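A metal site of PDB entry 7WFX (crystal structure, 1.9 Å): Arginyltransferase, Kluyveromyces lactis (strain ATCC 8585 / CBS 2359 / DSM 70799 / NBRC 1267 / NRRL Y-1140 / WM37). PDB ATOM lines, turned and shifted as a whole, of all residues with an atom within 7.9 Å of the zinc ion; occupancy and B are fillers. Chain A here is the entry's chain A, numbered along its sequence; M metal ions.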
ATOM      1  N   ALA A  23       6.754   2.119  26.846  1.00  0.00           N
ATOM      2  CA  ALA A  23       5.473   2.714  26.484  1.00  0.00           C
ATOM      3  C   ALA A  23       5.640   4.168  26.064  1.00  0.00           C
ATOM      4  O   ALA A  23       4.848   4.699  25.274  1.00  0.00           O
ATOM      5  CB  ALA A  23       4.517   2.633  27.677  1.00  0.00           C
ATOM      6  N   ASP A  24       6.629   4.848  26.626  1.00  0.00           N
ATOM      7  CA  ASP A  24       7.042   6.141  26.140  1.00  0.00           C
ATOM      8  C   ASP A  24       8.155   5.897  25.126  1.00  0.00           C
ATOM      9  O   ASP A  24       9.240   5.458  25.522  1.00  0.00           O
ATOM     10  CB  ASP A  24       7.533   6.990  27.315  1.00  0.00           C
ATOM     11  CG  ASP A  24       8.045   8.347  26.892  1.00  0.00           C
ATOM     12  OD1 ASP A  24       8.086   8.625  25.670  1.00  0.00           O
ATOM     13  OD2 ASP A  24       8.301   9.159  27.802  1.00  0.00           O
ATOM     14  N   LYS A  26       6.028   4.306  22.667  1.00  0.00           N
ATOM     15  CA  LYS A  26       5.367   3.344  21.802  1.00  0.00           C
ATOM     16  C   LYS A  26       3.849   3.383  21.933  1.00  0.00           C
ATOM     17  O   LYS A  26       3.151   3.075  20.966  1.00  0.00           O
ATOM     18  CB  LYS A  26       5.850   1.932  22.099  1.00  0.00           C
ATOM     19  CG  LYS A  26       5.271   0.917  21.137  1.00  0.00           C
ATOM     20  CD  LYS A  26       5.831  -0.474  21.385  1.00  0.00           C
ATOM     21  CE  LYS A  26       4.733  -1.550  21.392  1.00  0.00           C
ATOM     22  NZ  LYS A  26       5.320  -2.915  21.479  1.00  0.00           N
ATOM     23  N   CYS A  27       3.317   3.683  23.126  1.00  0.00           N
ATOM     24  CA  CYS A  27       1.875   3.637  23.344  1.00  0.00           C
ATOM     25  C   CYS A  27       1.245   4.954  22.925  1.00  0.00           C
ATOM     26  O   CYS A  27       1.487   5.984  23.566  1.00  0.00           O
ATOM     27  CB  CYS A  27       1.511   3.339  24.796  1.00  0.00           C
ATOM     28  SG  CYS A  27      -0.323   3.273  25.057  1.00  0.00           S
ATOM     29  N   GLY A  28       0.421   4.912  21.885  1.00  0.00           N
ATOM     30  CA  GLY A  28      -0.323   6.074  21.417  1.00  0.00           C
ATOM     31  C   GLY A  28      -1.483   6.488  22.304  1.00  0.00           C
ATOM     32  O   GLY A  28      -2.048   7.562  22.071  1.00  0.00           O
ATOM     33  N   TYR A  29      -1.840   5.689  23.304  1.00  0.00           N
ATOM     34  CA  TYR A  29      -2.933   6.069  24.184  1.00  0.00           C
ATOM     35  C   TYR A  29      -2.470   6.826  25.412  1.00  0.00           C
ATOM     36  O   TYR A  29      -3.138   7.781  25.832  1.00  0.00           O
ATOM     37  CB  TYR A  29      -3.690   4.819  24.651  1.00  0.00           C
ATOM     38  CG  TYR A  29      -4.078   3.887  23.543  1.00  0.00           C
ATOM     39  CD1 TYR A  29      -5.038   4.247  22.605  1.00  0.00           C
ATOM     40  CD2 TYR A  29      -3.525   2.638  23.441  1.00  0.00           C
ATOM     41  CE1 TYR A  29      -5.412   3.384  21.598  1.00  0.00           C
ATOM     42  CE2 TYR A  29      -3.884   1.763  22.444  1.00  0.00           C
ATOM     43  CZ  TYR A  29      -4.830   2.156  21.516  1.00  0.00           C
ATOM     44  OH  TYR A  29      -5.184   1.287  20.531  1.00  0.00           O
ATOM     45  N   CYS A  30      -1.356   6.411  26.038  1.00  0.00           N
ATOM     46  CA  CYS A  30      -0.881   7.070  27.239  1.00  0.00           C
ATOM     47  C   CYS A  30       0.496   7.687  27.105  1.00  0.00           C
ATOM     48  O   CYS A  30       0.901   8.418  28.011  1.00  0.00           O
ATOM     49  CB  CYS A  30      -0.863   6.099  28.446  1.00  0.00           C
ATOM     50  SG  CYS A  30       0.478   4.890  28.452  1.00  0.00           S
ATOM     51  N   ASN A  31       1.241   7.395  26.039  1.00  0.00           N
ATOM     52  CA  ASN A  31       2.627   7.863  25.898  1.00  0.00           C
ATOM     53  C   ASN A  31       3.510   7.472  27.088  1.00  0.00           C
ATOM     54  O   ASN A  31       4.494   8.130  27.374  1.00  0.00           O
ATOM     55  CB  ASN A  31       2.642   9.375  25.710  1.00  0.00           C
ATOM     56  CG  ASN A  31       1.769   9.801  24.539  1.00  0.00           C
ATOM     57  OD1 ASN A  31       1.954   9.307  23.427  1.00  0.00           O
ATOM     58  ND2 ASN A  31       0.784  10.664  24.784  1.00  0.00           N
ATOM     59  N   GLY A  32       3.154   6.405  27.793  1.00  0.00           N
ATOM     60  CA  GLY A  32       3.943   6.011  28.953  1.00  0.00           C
ATOM     61  C   GLY A  32       3.711   6.835  30.191  1.00  0.00           C
ATOM     62  O   GLY A  32       4.445   6.665  31.162  1.00  0.00           O
ATOM     63  N   LYS A  33       2.695   7.705  30.196  1.00  0.00           N
ATOM     64  CA  LYS A  33       2.416   8.602  31.318  1.00  0.00           C
ATOM     65  C   LYS A  33       1.167   8.089  32.011  1.00  0.00           C
ATOM     66  O   LYS A  33       0.082   8.107  31.423  1.00  0.00           O
ATOM     67  CB  LYS A  33       2.205  10.041  30.856  1.00  0.00           C
ATOM     68  CG  LYS A  33       3.227  10.550  29.862  1.00  0.00           C
ATOM     69  CD  LYS A  33       4.614  10.480  30.429  1.00  0.00           C
ATOM     70  CE  LYS A  33       5.633  11.171  29.547  1.00  0.00           C
ATOM     71  NZ  LYS A  33       5.482  10.759  28.110  1.00  0.00           N
ATOM     72  N   LYS A  34       1.304   7.643  33.240  1.00  0.00           N
ATOM     73  CA  LYS A  34       0.153   7.233  34.008  1.00  0.00           C
ATOM     74  C   LYS A  34       0.239   7.760  35.424  1.00  0.00           C
ATOM     75  O   LYS A  34       1.326   7.825  36.017  1.00  0.00           O
ATOM     76  CB  LYS A  34       0.038   5.695  34.001  1.00  0.00           C
ATOM     77  CG  LYS A  34      -0.407   5.145  32.643  1.00  0.00           C
ATOM     78  CD  LYS A  34      -1.543   4.165  32.868  1.00  0.00           C
ATOM     79  CE  LYS A  34      -2.207   3.758  31.592  1.00  0.00           C
ATOM     80  NZ  LYS A  34      -3.311   4.621  31.157  1.00  0.00           N
ATOM     81  N   LEU A  58       7.195   1.581  32.339  1.00  0.00           N
ATOM     82  CA  LEU A  58       6.069   0.920  31.700  1.00  0.00           C
ATOM     83  C   LEU A  58       6.434   0.519  30.277  1.00  0.00           C
ATOM     84  O   LEU A  58       7.166   1.219  29.578  1.00  0.00           O
ATOM     85  CB  LEU A  58       4.864   1.832  31.678  1.00  0.00           C
ATOM     86  CG  LEU A  58       4.140   2.002  33.017  1.00  0.00           C
ATOM     87  CD1 LEU A  58       2.959   2.892  32.776  1.00  0.00           C
ATOM     88  CD2 LEU A  58       3.708   0.684  33.601  1.00  0.00           C
ATOM     89  N   GLN A  59       5.879  -0.618  29.868  1.00  0.00           N
ATOM     90  CA  GLN A  59       6.108  -1.186  28.558  1.00  0.00           C
ATOM     91  C   GLN A  59       4.800  -1.265  27.803  1.00  0.00           C
ATOM     92  O   GLN A  59       3.734  -1.483  28.397  1.00  0.00           O
ATOM     93  CB  GLN A  59       6.695  -2.604  28.657  1.00  0.00           C
ATOM     94  CG  GLN A  59       7.980  -2.711  29.456  1.00  0.00           C
ATOM     95  CD  GLN A  59       9.107  -1.920  28.801  1.00  0.00           C
ATOM     96  OE1 GLN A  59       9.640  -2.303  27.773  1.00  0.00           O
ATOM     97  NE2 GLN A  59       9.429  -0.819  29.371  1.00  0.00           N
ATOM     98  N   SER A  60       4.875  -1.135  26.496  1.00  0.00           N
ATOM     99  CA  SER A  60       3.743  -1.434  25.624  1.00  0.00           C
ATOM    100  C   SER A  60       4.075  -2.711  24.872  1.00  0.00           C
ATOM    101  O   SER A  60       5.178  -2.846  24.332  1.00  0.00           O
ATOM    102  CB  SER A  60       3.451  -0.288  24.657  1.00  0.00           C
ATOM    103  OG  SER A  60       2.279  -0.558  23.895  1.00  0.00           O
ATOM    104  N   ASN A  98       1.004  -4.754  29.753  1.00  0.00           N
ATOM    105  CA  ASN A  98       0.858  -3.517  28.986  1.00  0.00           C
ATOM    106  C   ASN A  98       0.554  -2.326  29.895  1.00  0.00           C
ATOM    107  O   ASN A  98      -0.102  -2.458  30.932  1.00  0.00           O
ATOM    108  CB  ASN A  98      -0.260  -3.688  27.935  1.00  0.00           C
ATOM    109  CG  ASN A  98      -0.117  -2.755  26.763  1.00  0.00           C
ATOM    110  OD1 ASN A  98       0.890  -2.763  26.061  1.00  0.00           O
ATOM    111  ND2 ASN A  98      -1.122  -1.925  26.547  1.00  0.00           N
ATOM    112  N   CYS A  99       1.055  -1.160  29.522  1.00  0.00           N
ATOM    113  CA  CYS A  99       0.752   0.080  30.241  1.00  0.00           C
ATOM    114  C   CYS A  99      -0.739   0.294  30.411  1.00  0.00           C
ATOM    115  O   CYS A  99      -1.205   0.645  31.498  1.00  0.00           O
ATOM    116  CB  CYS A  99       1.347   1.279  29.489  1.00  0.00           C
ATOM    117  SG  CYS A  99       1.037   1.213  27.698  1.00  0.00           S
ATOM    118  N   CYS A 100      -1.508   0.122  29.335  1.00  0.00           N
ATOM    119  CA  CYS A 100      -2.946   0.372  29.319  1.00  0.00           C
ATOM    120  C   CYS A 100      -3.745  -0.925  29.230  1.00  0.00           C
ATOM    121  O   CYS A 100      -3.384  -1.846  28.509  1.00  0.00           O
ATOM    122  CB  CYS A 100      -3.318   1.270  28.127  1.00  0.00           C
ATOM    123  SG  CYS A 100      -2.591   2.950  28.184  1.00  0.00           S
ATOM    124  N   ARG A 101      -4.879  -0.965  29.932  1.00  0.00           N
ATOM    125  CA  ARG A 101      -5.739  -2.150  29.925  1.00  0.00           C
ATOM    126  C   ARG A 101      -6.760  -1.990  28.806  1.00  0.00           C
ATOM    127  O   ARG A 101      -7.687  -1.173  28.908  1.00  0.00           O
ATOM    128  CB  ARG A 101      -6.405  -2.335  31.294  1.00  0.00           C
ATOM    129  CG  ARG A 101      -6.578  -3.810  31.694  1.00  0.00           C
ATOM    130  CD  ARG A 101      -5.253  -4.478  32.003  1.00  0.00           C
ATOM    131  NE  ARG A 101      -4.551  -3.662  32.977  1.00  0.00           N
ATOM    132  CZ  ARG A 101      -3.297  -3.254  32.871  1.00  0.00           C
ATOM    133  NH1 ARG A 101      -2.465  -3.820  32.008  1.00  0.00           N
ATOM    134  NH2 ARG A 101      -2.881  -2.234  33.603  1.00  0.00           N
ATOM    135  N   LEU A 102      -6.591  -2.772  27.731  1.00  0.00           N
ATOM    136  CA  LEU A 102      -7.467  -2.748  26.563  1.00  0.00           C
ATOM    137  C   LEU A 102      -8.453  -3.917  26.630  1.00  0.00           C
ATOM    138  O   LEU A 102      -8.050  -5.079  26.632  1.00  0.00           O
ATOM    139  CB  LEU A 102      -6.668  -2.846  25.274  1.00  0.00           C
ATOM    140  CG  LEU A 102      -6.037  -1.547  24.794  1.00  0.00           C
ATOM    141  CD1 LEU A 102      -4.963  -1.098  25.751  1.00  0.00           C
ATOM    142  CD2 LEU A 102      -5.496  -1.697  23.369  1.00  0.00           C
ATOM    143  N   ILE A 299     -10.598   1.387  26.634  1.00  0.00           N
ATOM    144  CA  ILE A 299      -9.616   1.709  27.680  1.00  0.00           C
ATOM    145  C   ILE A 299     -10.279   2.715  28.617  1.00  0.00           C
ATOM    146  O   ILE A 299     -10.546   3.855  28.233  1.00  0.00           O
ATOM    147  CB  ILE A 299      -8.321   2.302  27.112  1.00  0.00           C
ATOM    148  CG1 ILE A 299      -7.721   1.419  26.029  1.00  0.00           C
ATOM    149  CG2 ILE A 299      -7.280   2.538  28.226  1.00  0.00           C
ATOM    150  CD1 ILE A 299      -6.519   2.117  25.328  1.00  0.00           C
ATOM    151  N   ASP A 301      -9.449   4.569  31.040  1.00  0.00           N
ATOM    152  CA  ASP A 301      -8.846   5.851  31.392  1.00  0.00           C
ATOM    153  C   ASP A 301      -8.286   6.620  30.209  1.00  0.00           C
ATOM    154  O   ASP A 301      -7.535   7.578  30.411  1.00  0.00           O
ATOM    155  CB  ASP A 301      -7.771   5.646  32.490  1.00  0.00           C
ATOM    156  CG  ASP A 301      -6.519   4.922  31.996  1.00  0.00           C
ATOM    157  OD1 ASP A 301      -6.353   4.703  30.789  1.00  0.00           O
ATOM    158  OD2 ASP A 301      -5.632   4.601  32.846  1.00  0.00           O
ATOM    159  N   CYS A 302      -8.670   6.281  28.975  1.00  0.00           N
ATOM    160  CA  CYS A 302      -8.242   7.034  27.793  1.00  0.00           C
ATOM    161  C   CYS A 302      -9.446   7.710  27.133  1.00  0.00           C
ATOM    162  O   CYS A 302     -10.313   7.021  26.571  1.00  0.00           O
ATOM    163  CB  CYS A 302      -7.549   6.103  26.785  1.00  0.00           C
ATOM    164  SG  CYS A 302      -6.965   6.843  25.251  1.00  0.00           S
ATOM    165  N   ASN A 336      -7.523   1.298  35.782  1.00  0.00           N
ATOM    166  CA  ASN A 336      -6.706   0.572  34.793  1.00  0.00           C
ATOM    167  C   ASN A 336      -6.360  -0.853  35.245  1.00  0.00           C
ATOM    168  O   ASN A 336      -5.410  -1.469  34.715  1.00  0.00           O
ATOM    169  CB  ASN A 336      -5.435   1.396  34.508  1.00  0.00           C
ATOM    170  CG  ASN A 336      -4.710   1.037  33.213  1.00  0.00           C
ATOM    171  OD1 ASN A 336      -5.297   0.847  32.145  1.00  0.00           O
ATOM    172  ND2 ASN A 336      -3.380   0.986  33.314  1.00  0.00           N
HETATM  173 ZN    ZN M   1      -0.445   3.038  27.396  1.00  0.00          ZN
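N of Gly 32 lies close to SG of Cys 30, 3.1 Å away.
SG of Cys 100 sits close to NZ of Lys 34 (3.5 Å).
The backbone carbonyl oxygen (O) of Cys 99 is in hydrogen-bond range of the side-chain amide nitrogen (ND2) of Asn 336 (2.9 Å).
The side-chain amide nitrogen (ND2) of Asn 98 is in hydrogen-bond range of the backbone carbonyl oxygen (O) of Cys 100 (3.0 Å).
The side-chain sulfur (SG) of Cys 27 lies close to the backbone NH (N) of Tyr 29, 3.3 Å away.
The backbone carbonyl oxygen (O) of Cys 27 lies close to the side-chain amide oxygen (OD1) of Asn 31.
The backbone NH of Cys 99 is in hydrogen-bond range of the backbone carbonyl oxygen of Gln 59, at 2.9 Å.
The nearest printed residue that does not touch the zinc ion is Lys 34 (4.6 Å).
The zinc ion is bound by the side-chain sulfur (SG) of Cys 100, the side-chain sulfur (SG) of Cys 30, the side-chain sulfur (SG) of Cys 27 and the side-chain sulfur (SG) of Cys 99.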
